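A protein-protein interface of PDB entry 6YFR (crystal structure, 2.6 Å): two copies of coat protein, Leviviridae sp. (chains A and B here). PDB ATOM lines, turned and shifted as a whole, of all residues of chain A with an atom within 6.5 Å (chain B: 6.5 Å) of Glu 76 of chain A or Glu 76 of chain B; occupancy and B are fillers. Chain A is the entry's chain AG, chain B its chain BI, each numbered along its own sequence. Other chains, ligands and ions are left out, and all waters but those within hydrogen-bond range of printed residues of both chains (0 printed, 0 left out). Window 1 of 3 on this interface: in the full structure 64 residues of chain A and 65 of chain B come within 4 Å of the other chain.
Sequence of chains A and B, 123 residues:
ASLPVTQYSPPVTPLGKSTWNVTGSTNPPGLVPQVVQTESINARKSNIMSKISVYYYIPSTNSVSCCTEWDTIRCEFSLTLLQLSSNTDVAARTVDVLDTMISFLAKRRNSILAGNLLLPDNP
The backbone carbonyl oxygen of Ile 52 of chain A is in hydrogen-bond range of the backbone NH of Phe 77 of chain A, at 2.9 Å. The side-chain hydroxyl of Ser 53 of chain A lies close to the side-chain carboxylate of Glu 76 of chain A, at 3.4 Å. OE2 of Glu 76 of chain A is in hydrogen-bond range of OH of Tyr 55 of chain A (3.3 Å). O of Ile 52 of chain B sits at hydrogen-bond distance from N of Phe 77 of chain B, at 2.9 Å. The side-chain hydroxyl (OG) of Ser 53 of chain B sits close to the side-chain carboxylate (OE2) of Glu 76 of chain B (3.4 Å). The backbone NH of Val 54 of chain B lies within hydrogen-bond range of the backbone carbonyl oxygen of Cys 75 of chain B.
Of the 13 printed residues of chain A, 8 touch a printed residue of chain B. Of the 13 printed residues of chain B, 8 touch a printed residue of chain A. Hydrophobic or aromatic side chains of chain B that line the printed part of chain A: Ile 52, Phe 77, Leu 79 and Met 101. Among the printed residues, 21 pairs touch across the chains. Among the printed residues, no Asp or Glu carboxylate lies within 4 Å of a Lys or Arg side-chain nitrogen of the other chain.
The side-chain sulfur (SG) of Cys 75 of chain A sits close to the backbone carbonyl oxygen (O) of Ser 78 of chain B (3.5 Å). The backbone carbonyl oxygen of Ser 78 of chain B is in hydrogen-bond range of the backbone NH of Glu 76 of chain A (2.8 Å). The side-chain sulfur (SG) of Cys 75 of chain B sits close to the backbone carbonyl oxygen (O) of Ser 78 of chain A, 3.5 Å away. The backbone NH (N) of Ser 78 of chain A sits at hydrogen-bond distance from the backbone carbonyl oxygen (O) of Glu 76 of chain B.
Of chain B, only Glu 76, Phe 77 and Ser 78 come within 4 Å of Glu 76 of chain A. Glu 76 of chain B touches three residues of chain A. Printed residues of chain B within 4 Å of Arg 74 of chain A: Ser 78 and Leu 79. Of the printed residues of chain B, Met 101 of chain A touches Ile 52, Cys 75 and Phe 77. Of the printed residues of chain B, Ser 78 of chain A touches Arg 74 (3.9 Å), Cys 75 (3.1 Å) and Glu 76 (2.8 Å). The nearest residue of chain B that does not touch Glu 76 of chain A is Met 101 of chain B (4.8 Å). The nearest residue of chain A that does not touch Glu 76 of chain B is Met 101 of chain A (4.8 Å).
Cys 75 of chain A touches Ser 78 of chain B, and with the chains exchanged Ser 78 of chain A touches Cys 75 of chain B. Cys 75 of chain A touches Leu 79 of chain B, and with the chains exchanged Leu 79 of chain A touches Cys 75 of chain B. Glu 76 of chain A touches Phe 77 of chain B, and with the chains exchanged Phe 77 of chain A touches Glu 76 of chain B. Phe 77 of chain A touches Met 101 of chain B, and with the chains exchanged Met 101 of chain A touches Phe 77 of chain B. Of the 21 pairs that touch across the chains among the printed residues, 21 have their exchanged pair printed and touching as well.
Ile 52 of chain A touches Met 101 of chain B (CB to CE, 3.4 Å). Arg 74 of chain A touches Ser 78 of chain B (O to O, 3.9 Å). Cys 75 of chain A touches Leu 79 of chain B. SG of Cys 75 of chain A touches CG of Met 101 of chain B (3.7 Å). O of Glu 76 of chain A touches O of Glu 76 of chain B, at 3.9 Å. Phe 77 of chain B touches Glu 76 of chain A (CA to O, 3.0 Å). Glu 76 of chain B touches Phe 77 of chain A (O to CA, 3.0 Å). O of Arg 74 of chain B touches O of Ser 78 of chain A, 3.9 Å away. CB of Cys 75 of chain B touches CD1 of Leu 79 of chain A (3.8 Å). Met 101 of chain A touches Phe 77 of chain B (CE to CB, 3.7 Å).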
ATOM      1  N   VAL A  36     -16.285  -8.441 -22.823  1.00  0.00           N
ATOM      2  CA  VAL A  36     -16.425  -7.333 -23.758  1.00  0.00           C
ATOM      3  C   VAL A  36     -17.792  -6.699 -23.549  1.00  0.00           C
ATOM      4  O   VAL A  36     -18.816  -7.388 -23.624  1.00  0.00           O
ATOM      5  CB  VAL A  36     -16.257  -7.796 -25.213  1.00  0.00           C
ATOM      6  CG1 VAL A  36     -16.354  -6.613 -26.162  1.00  0.00           C
ATOM      7  CG2 VAL A  36     -14.935  -8.524 -25.387  1.00  0.00           C
ATOM      8  N   LYS A  51     -24.537  -4.717 -24.835  1.00  0.00           N
ATOM      9  CA  LYS A  51     -24.160  -6.121 -24.827  1.00  0.00           C
ATOM     10  C   LYS A  51     -23.005  -6.368 -23.867  1.00  0.00           C
ATOM     11  O   LYS A  51     -22.106  -5.535 -23.718  1.00  0.00           O
ATOM     12  CB  LYS A  51     -23.760  -6.595 -26.232  1.00  0.00           C
ATOM     13  CG  LYS A  51     -24.877  -6.552 -27.264  1.00  0.00           C
ATOM     14  CD  LYS A  51     -24.365  -7.011 -28.626  1.00  0.00           C
ATOM     15  CE  LYS A  51     -25.458  -6.945 -29.680  1.00  0.00           C
ATOM     16  NZ  LYS A  51     -24.967  -7.368 -31.021  1.00  0.00           N
ATOM     17  N   ILE A  52     -23.042  -7.531 -23.221  1.00  0.00           N
ATOM     18  CA  ILE A  52     -21.918  -8.054 -22.452  1.00  0.00           C
ATOM     19  C   ILE A  52     -21.627  -9.461 -22.958  1.00  0.00           C
ATOM     20  O   ILE A  52     -22.550 -10.262 -23.143  1.00  0.00           O
ATOM     21  CB  ILE A  52     -22.199  -8.074 -20.935  1.00  0.00           C
ATOM     22  CG1 ILE A  52     -22.600  -6.690 -20.426  1.00  0.00           C
ATOM     23  CG2 ILE A  52     -20.978  -8.573 -20.173  1.00  0.00           C
ATOM     24  CD1 ILE A  52     -21.430  -5.780 -20.164  1.00  0.00           C
ATOM     25  N   SER A  53     -20.352  -9.765 -23.171  1.00  0.00           N
ATOM     26  CA  SER A  53     -19.944 -11.049 -23.722  1.00  0.00           C
ATOM     27  C   SER A  53     -18.754 -11.579 -22.941  1.00  0.00           C
ATOM     28  O   SER A  53     -17.757 -10.874 -22.766  1.00  0.00           O
ATOM     29  CB  SER A  53     -19.586 -10.918 -25.205  1.00  0.00           C
ATOM     30  OG  SER A  53     -20.690 -10.429 -25.950  1.00  0.00           O
ATOM     31  N   VAL A  54     -18.859 -12.813 -22.468  1.00  0.00           N
ATOM     32  CA  VAL A  54     -17.772 -13.481 -21.765  1.00  0.00           C
ATOM     33  C   VAL A  54     -17.313 -14.635 -22.641  1.00  0.00           C
ATOM     34  O   VAL A  54     -18.085 -15.571 -22.905  1.00  0.00           O
ATOM     35  CB  VAL A  54     -18.204 -13.968 -20.375  1.00  0.00           C
ATOM     36  CG1 VAL A  54     -17.043 -14.654 -19.686  1.00  0.00           C
ATOM     37  CG2 VAL A  54     -18.710 -12.802 -19.545  1.00  0.00           C
ATOM     38  N   TYR A  55     -16.067 -14.552 -23.107  1.00  0.00           N
ATOM     39  CA  TYR A  55     -15.429 -15.603 -23.891  1.00  0.00           C
ATOM     40  C   TYR A  55     -14.357 -16.240 -23.015  1.00  0.00           C
ATOM     41  O   TYR A  55     -13.353 -15.594 -22.691  1.00  0.00           O
ATOM     42  CB  TYR A  55     -14.814 -15.039 -25.171  1.00  0.00           C
ATOM     43  CG  TYR A  55     -15.749 -14.194 -26.006  1.00  0.00           C
ATOM     44  CD1 TYR A  55     -16.742 -14.779 -26.779  1.00  0.00           C
ATOM     45  CD2 TYR A  55     -15.625 -12.811 -26.038  1.00  0.00           C
ATOM     46  CE1 TYR A  55     -17.597 -14.012 -27.550  1.00  0.00           C
ATOM     47  CE2 TYR A  55     -16.474 -12.033 -26.808  1.00  0.00           C
ATOM     48  CZ  TYR A  55     -17.457 -12.639 -27.561  1.00  0.00           C
ATOM     49  OH  TYR A  55     -18.304 -11.869 -28.326  1.00  0.00           O
ATOM     50  N   ARG A  74     -19.035 -19.505 -24.174  1.00  0.00           N
ATOM     51  CA  ARG A  74     -19.559 -18.190 -24.518  1.00  0.00           C
ATOM     52  C   ARG A  74     -20.800 -17.899 -23.692  1.00  0.00           C
ATOM     53  O   ARG A  74     -21.712 -18.734 -23.607  1.00  0.00           O
ATOM     54  CB  ARG A  74     -19.905 -18.094 -26.007  1.00  0.00           C
ATOM     55  CG  ARG A  74     -18.773 -17.612 -26.884  1.00  0.00           C
ATOM     56  CD  ARG A  74     -19.249 -17.366 -28.306  1.00  0.00           C
ATOM     57  NE  ARG A  74     -18.150 -16.973 -29.183  1.00  0.00           N
ATOM     58  CZ  ARG A  74     -17.389 -17.828 -29.859  1.00  0.00           C
ATOM     59  NH1 ARG A  74     -17.610 -19.133 -29.765  1.00  0.00           N
ATOM     60  NH2 ARG A  74     -16.410 -17.380 -30.632  1.00  0.00           N
ATOM     61  N   CYS A  75     -20.832 -16.708 -23.096  1.00  0.00           N
ATOM     62  CA  CYS A  75     -22.006 -16.221 -22.384  1.00  0.00           C
ATOM     63  C   CYS A  75     -22.324 -14.818 -22.880  1.00  0.00           C
ATOM     64  O   CYS A  75     -21.511 -13.902 -22.717  1.00  0.00           O
ATOM     65  CB  CYS A  75     -21.772 -16.228 -20.873  1.00  0.00           C
ATOM     66  SG  CYS A  75     -23.216 -15.773 -19.900  1.00  0.00           S
ATOM     67  N   GLU A  76     -23.503 -14.651 -23.472  1.00  0.00           N
ATOM     68  CA  GLU A  76     -23.903 -13.408 -24.119  1.00  0.00           C
ATOM     69  C   GLU A  76     -25.111 -12.801 -23.421  1.00  0.00           C
ATOM     70  O   GLU A  76     -25.992 -13.514 -22.930  1.00  0.00           O
ATOM     71  CB  GLU A  76     -24.246 -13.633 -25.601  1.00  0.00           C
ATOM     72  CG  GLU A  76     -23.105 -14.163 -26.455  1.00  0.00           C
ATOM     73  CD  GLU A  76     -22.121 -13.082 -26.860  1.00  0.00           C
ATOM     74  OE1 GLU A  76     -22.328 -11.911 -26.474  1.00  0.00           O
ATOM     75  OE2 GLU A  76     -21.141 -13.404 -27.569  1.00  0.00           O
ATOM     76  N   PHE A  77     -25.149 -11.469 -23.406  1.00  0.00           N
ATOM     77  CA  PHE A  77     -26.260 -10.693 -22.875  1.00  0.00           C
ATOM     78  C   PHE A  77     -26.456  -9.469 -23.754  1.00  0.00           C
ATOM     79  O   PHE A  77     -25.483  -8.810 -24.134  1.00  0.00           O
ATOM     80  CB  PHE A  77     -25.994 -10.267 -21.424  1.00  0.00           C
ATOM     81  CG  PHE A  77     -26.872  -9.138 -20.933  1.00  0.00           C
ATOM     82  CD1 PHE A  77     -28.027  -9.405 -20.220  1.00  0.00           C
ATOM     83  CD2 PHE A  77     -26.521  -7.811 -21.157  1.00  0.00           C
ATOM     84  CE1 PHE A  77     -28.828  -8.370 -19.755  1.00  0.00           C
ATOM     85  CE2 PHE A  77     -27.321  -6.776 -20.701  1.00  0.00           C
ATOM     86  CZ  PHE A  77     -28.476  -7.055 -19.999  1.00  0.00           C
ATOM     87  N   SER A  78     -27.713  -9.156 -24.049  1.00  0.00           N
ATOM     88  CA  SER A  78     -28.051  -7.975 -24.830  1.00  0.00           C
ATOM     89  C   SER A  78     -29.319  -7.343 -24.277  1.00  0.00           C
ATOM     90  O   SER A  78     -30.194  -8.033 -23.750  1.00  0.00           O
ATOM     91  CB  SER A  78     -28.249  -8.308 -26.313  1.00  0.00           C
ATOM     92  OG  SER A  78     -29.485  -8.970 -26.521  1.00  0.00           O
ATOM     93  N   LEU A  79     -29.409  -6.021 -24.411  1.00  0.00           N
ATOM     94  CA  LEU A  79     -30.567  -5.255 -23.961  1.00  0.00           C
ATOM     95  C   LEU A  79     -30.817  -4.120 -24.942  1.00  0.00           C
ATOM     96  O   LEU A  79     -29.872  -3.440 -25.363  1.00  0.00           O
ATOM     97  CB  LEU A  79     -30.357  -4.700 -22.548  1.00  0.00           C
ATOM     98  CG  LEU A  79     -31.435  -3.772 -21.985  1.00  0.00           C
ATOM     99  CD1 LEU A  79     -32.765  -4.498 -21.846  1.00  0.00           C
ATOM    100  CD2 LEU A  79     -30.991  -3.196 -20.647  1.00  0.00           C
ATOM    101  N   MET A 101     -34.489 -10.148 -15.878  1.00  0.00           N
ATOM    102  CA  MET A 101     -33.400 -10.974 -16.391  1.00  0.00           C
ATOM    103  C   MET A 101     -32.532 -11.504 -15.256  1.00  0.00           C
ATOM    104  O   MET A 101     -32.228 -12.703 -15.191  1.00  0.00           O
ATOM    105  CB  MET A 101     -32.559 -10.159 -17.376  1.00  0.00           C
ATOM    106  CG  MET A 101     -31.421 -10.924 -18.015  1.00  0.00           C
ATOM    107  SD  MET A 101     -32.026 -12.227 -19.100  1.00  0.00           S
ATOM    108  CE  MET A 101     -31.536 -13.641 -18.151  1.00  0.00           C
ATOM    109  N   VAL B  36     -38.907 -16.251 -21.735  1.00  0.00           N
ATOM    110  CA  VAL B  36     -38.775 -17.548 -22.386  1.00  0.00           C
ATOM    111  C   VAL B  36     -37.402 -18.113 -22.054  1.00  0.00           C
ATOM    112  O   VAL B  36     -36.382 -17.459 -22.305  1.00  0.00           O
ATOM    113  CB  VAL B  36     -38.966 -17.439 -23.906  1.00  0.00           C
ATOM    114  CG1 VAL B  36     -38.877 -18.812 -24.552  1.00  0.00           C
ATOM    115  CG2 VAL B  36     -40.293 -16.775 -24.227  1.00  0.00           C
ATOM    116  N   LYS B  51     -30.666 -20.331 -22.938  1.00  0.00           N
ATOM    117  CA  LYS B  51     -31.049 -18.965 -23.256  1.00  0.00           C
ATOM    118  C   LYS B  51     -32.192 -18.501 -22.363  1.00  0.00           C
ATOM    119  O   LYS B  51     -33.085 -19.277 -22.009  1.00  0.00           O
ATOM    120  CB  LYS B  51     -31.471 -18.835 -24.726  1.00  0.00           C
ATOM    121  CG  LYS B  51     -30.369 -19.118 -25.736  1.00  0.00           C
ATOM    122  CD  LYS B  51     -30.903 -18.993 -27.160  1.00  0.00           C
ATOM    123  CE  LYS B  51     -29.824 -19.304 -28.186  1.00  0.00           C
ATOM    124  NZ  LYS B  51     -30.337 -19.209 -29.580  1.00  0.00           N
ATOM    125  N   ILE B  52     -32.152 -17.219 -22.009  1.00  0.00           N
ATOM    126  CA  ILE B  52     -33.268 -16.530 -21.368  1.00  0.00           C
ATOM    127  C   ILE B  52     -33.572 -15.283 -22.186  1.00  0.00           C
ATOM    128  O   ILE B  52     -32.656 -14.547 -22.568  1.00  0.00           O
ATOM    129  CB  ILE B  52     -32.965 -16.154 -19.903  1.00  0.00           C
ATOM    130  CG1 ILE B  52     -32.550 -17.379 -19.089  1.00  0.00           C
ATOM    131  CG2 ILE B  52     -34.178 -15.492 -19.261  1.00  0.00           C
ATOM    132  CD1 ILE B  52     -33.713 -18.205 -18.603  1.00  0.00           C
ATOM    133  N   SER B  53     -34.853 -15.040 -22.447  1.00  0.00           N
ATOM    134  CA  SER B  53     -35.275 -13.923 -23.277  1.00  0.00           C
ATOM    135  C   SER B  53     -36.455 -13.224 -22.624  1.00  0.00           C
ATOM    136  O   SER B  53     -37.446 -13.871 -22.275  1.00  0.00           O
ATOM    137  CB  SER B  53     -35.652 -14.398 -24.683  1.00  0.00           C
ATOM    138  OG  SER B  53     -34.556 -15.046 -25.308  1.00  0.00           O
ATOM    139  N   VAL B  54     -36.349 -11.913 -22.457  1.00  0.00           N
ATOM    140  CA  VAL B  54     -37.429 -11.102 -21.915  1.00  0.00           C
ATOM    141  C   VAL B  54     -37.907 -10.186 -23.030  1.00  0.00           C
ATOM    142  O   VAL B  54     -37.144  -9.338 -23.518  1.00  0.00           O
ATOM    143  CB  VAL B  54     -36.981 -10.300 -20.684  1.00  0.00           C
ATOM    144  CG1 VAL B  54     -38.136  -9.473 -20.159  1.00  0.00           C
ATOM    145  CG2 VAL B  54     -36.458 -11.237 -19.611  1.00  0.00           C
ATOM    146  N   TYR B  55     -39.159 -10.378 -23.445  1.00  0.00           N
ATOM    147  CA  TYR B  55     -39.813  -9.542 -24.444  1.00  0.00           C
ATOM    148  C   TYR B  55     -40.876  -8.719 -23.727  1.00  0.00           C
ATOM    149  O   TYR B  55     -41.872  -9.271 -23.245  1.00  0.00           O
ATOM    150  CB  TYR B  55     -40.444 -10.393 -25.547  1.00  0.00           C
ATOM    151  CG  TYR B  55     -39.516 -11.408 -26.173  1.00  0.00           C
ATOM    152  CD1 TYR B  55     -38.537 -11.020 -27.077  1.00  0.00           C
ATOM    153  CD2 TYR B  55     -39.634 -12.760 -25.878  1.00  0.00           C
ATOM    154  CE1 TYR B  55     -37.689 -11.945 -27.659  1.00  0.00           C
ATOM    155  CE2 TYR B  55     -38.793 -13.697 -26.456  1.00  0.00           C
ATOM    156  CZ  TYR B  55     -37.823 -13.283 -27.345  1.00  0.00           C
ATOM    157  OH  TYR B  55     -36.982 -14.210 -27.920  1.00  0.00           O
ATOM    158  N   ARG B  74     -36.231  -5.811 -25.690  1.00  0.00           N
ATOM    159  CA  ARG B  74     -35.705  -7.169 -25.725  1.00  0.00           C
ATOM    160  C   ARG B  74     -34.452  -7.255 -24.871  1.00  0.00           C
ATOM    161  O   ARG B  74     -33.542  -6.422 -24.998  1.00  0.00           O
ATOM    162  CB  ARG B  74     -35.380  -7.612 -27.153  1.00  0.00           C
ATOM    163  CG  ARG B  74     -36.523  -8.288 -27.875  1.00  0.00           C
ATOM    164  CD  ARG B  74     -36.066  -8.861 -29.207  1.00  0.00           C
ATOM    165  NE  ARG B  74     -37.175  -9.451 -29.950  1.00  0.00           N
ATOM    166  CZ  ARG B  74     -37.949  -8.780 -30.798  1.00  0.00           C
ATOM    167  NH1 ARG B  74     -37.733  -7.489 -31.015  1.00  0.00           N
ATOM    168  NH2 ARG B  74     -38.936  -9.399 -31.429  1.00  0.00           N
ATOM    169  N   CYS B  75     -34.406  -8.273 -24.013  1.00  0.00           N
ATOM    170  CA  CYS B  75     -33.218  -8.577 -23.223  1.00  0.00           C
ATOM    171  C   CYS B  75     -32.901 -10.057 -23.380  1.00  0.00           C
ATOM    172  O   CYS B  75     -33.707 -10.910 -22.995  1.00  0.00           O
ATOM    173  CB  CYS B  75     -33.431  -8.215 -21.754  1.00  0.00           C
ATOM    174  SG  CYS B  75     -31.971  -8.427 -20.722  1.00  0.00           S
ATOM    175  N   GLU B  76     -31.729 -10.357 -23.935  1.00  0.00           N
ATOM    176  CA  GLU B  76     -31.333 -11.716 -24.277  1.00  0.00           C
ATOM    177  C   GLU B  76     -30.111 -12.140 -23.473  1.00  0.00           C
ATOM    178  O   GLU B  76     -29.227 -11.331 -23.177  1.00  0.00           O
ATOM    179  CB  GLU B  76     -31.011 -11.845 -25.775  1.00  0.00           C
ATOM    180  CG  GLU B  76     -32.167 -11.533 -26.713  1.00  0.00           C
ATOM    181  CD  GLU B  76     -33.151 -12.680 -26.837  1.00  0.00           C
ATOM    182  OE1 GLU B  76     -32.934 -13.728 -26.191  1.00  0.00           O
ATOM    183  OE2 GLU B  76     -34.143 -12.536 -27.587  1.00  0.00           O
ATOM    184  N   PHE B  77     -30.067 -13.431 -23.146  1.00  0.00           N
ATOM    185  CA  PHE B  77     -28.945 -14.060 -22.465  1.00  0.00           C
ATOM    186  C   PHE B  77     -28.755 -15.455 -23.035  1.00  0.00           C
ATOM    187  O   PHE B  77     -29.731 -16.187 -23.234  1.00  0.00           O
ATOM    188  CB  PHE B  77     -29.188 -14.132 -20.949  1.00  0.00           C
ATOM    189  CG  PHE B  77     -28.299 -15.113 -20.222  1.00  0.00           C
ATOM    190  CD1 PHE B  77     -27.134 -14.685 -19.607  1.00  0.00           C
ATOM    191  CD2 PHE B  77     -28.645 -16.455 -20.122  1.00  0.00           C
ATOM    192  CE1 PHE B  77     -26.321 -15.579 -18.924  1.00  0.00           C
ATOM    193  CE2 PHE B  77     -27.834 -17.353 -19.447  1.00  0.00           C
ATOM    194  CZ  PHE B  77     -26.670 -16.916 -18.848  1.00  0.00           C
ATOM    195  N   SER B  78     -27.501 -15.828 -23.266  1.00  0.00           N
ATOM    196  CA  SER B  78     -27.168 -17.158 -23.753  1.00  0.00           C
ATOM    197  C   SER B  78     -25.889 -17.640 -23.085  1.00  0.00           C
ATOM    198  O   SER B  78     -25.010 -16.845 -22.749  1.00  0.00           O
ATOM    199  CB  SER B  78     -26.993 -17.183 -25.275  1.00  0.00           C
ATOM    200  OG  SER B  78     -25.763 -16.587 -25.650  1.00  0.00           O
ATOM    201  N   LEU B  79     -25.794 -18.957 -22.905  1.00  0.00           N
ATOM    202  CA  LEU B  79     -24.627 -19.593 -22.306  1.00  0.00           C
ATOM    203  C   LEU B  79     -24.385 -20.928 -22.996  1.00  0.00           C
ATOM    204  O   LEU B  79     -25.332 -21.688 -23.232  1.00  0.00           O
ATOM    205  CB  LEU B  79     -24.814 -19.801 -20.799  1.00  0.00           C
ATOM    206  CG  LEU B  79     -23.723 -20.569 -20.050  1.00  0.00           C
ATOM    207  CD1 LEU B  79     -22.396 -19.830 -20.104  1.00  0.00           C
ATOM    208  CD2 LEU B  79     -24.146 -20.815 -18.607  1.00  0.00           C
ATOM    209  N   MET B 101     -20.616 -12.932 -15.659  1.00  0.00           N
ATOM    210  CA  MET B 101     -21.715 -12.251 -16.336  1.00  0.00           C
ATOM    211  C   MET B 101     -22.571 -11.470 -15.343  1.00  0.00           C
ATOM    212  O   MET B 101     -22.879 -10.289 -15.559  1.00  0.00           O
ATOM    213  CB  MET B 101     -22.565 -13.275 -17.089  1.00  0.00           C
ATOM    214  CG  MET B 101     -23.717 -12.685 -17.873  1.00  0.00           C
ATOM    215  SD  MET B 101     -23.133 -11.672 -19.242  1.00  0.00           S
ATOM    216  CE  MET B 101     -23.617 -10.075 -18.645  1.00  0.00           C
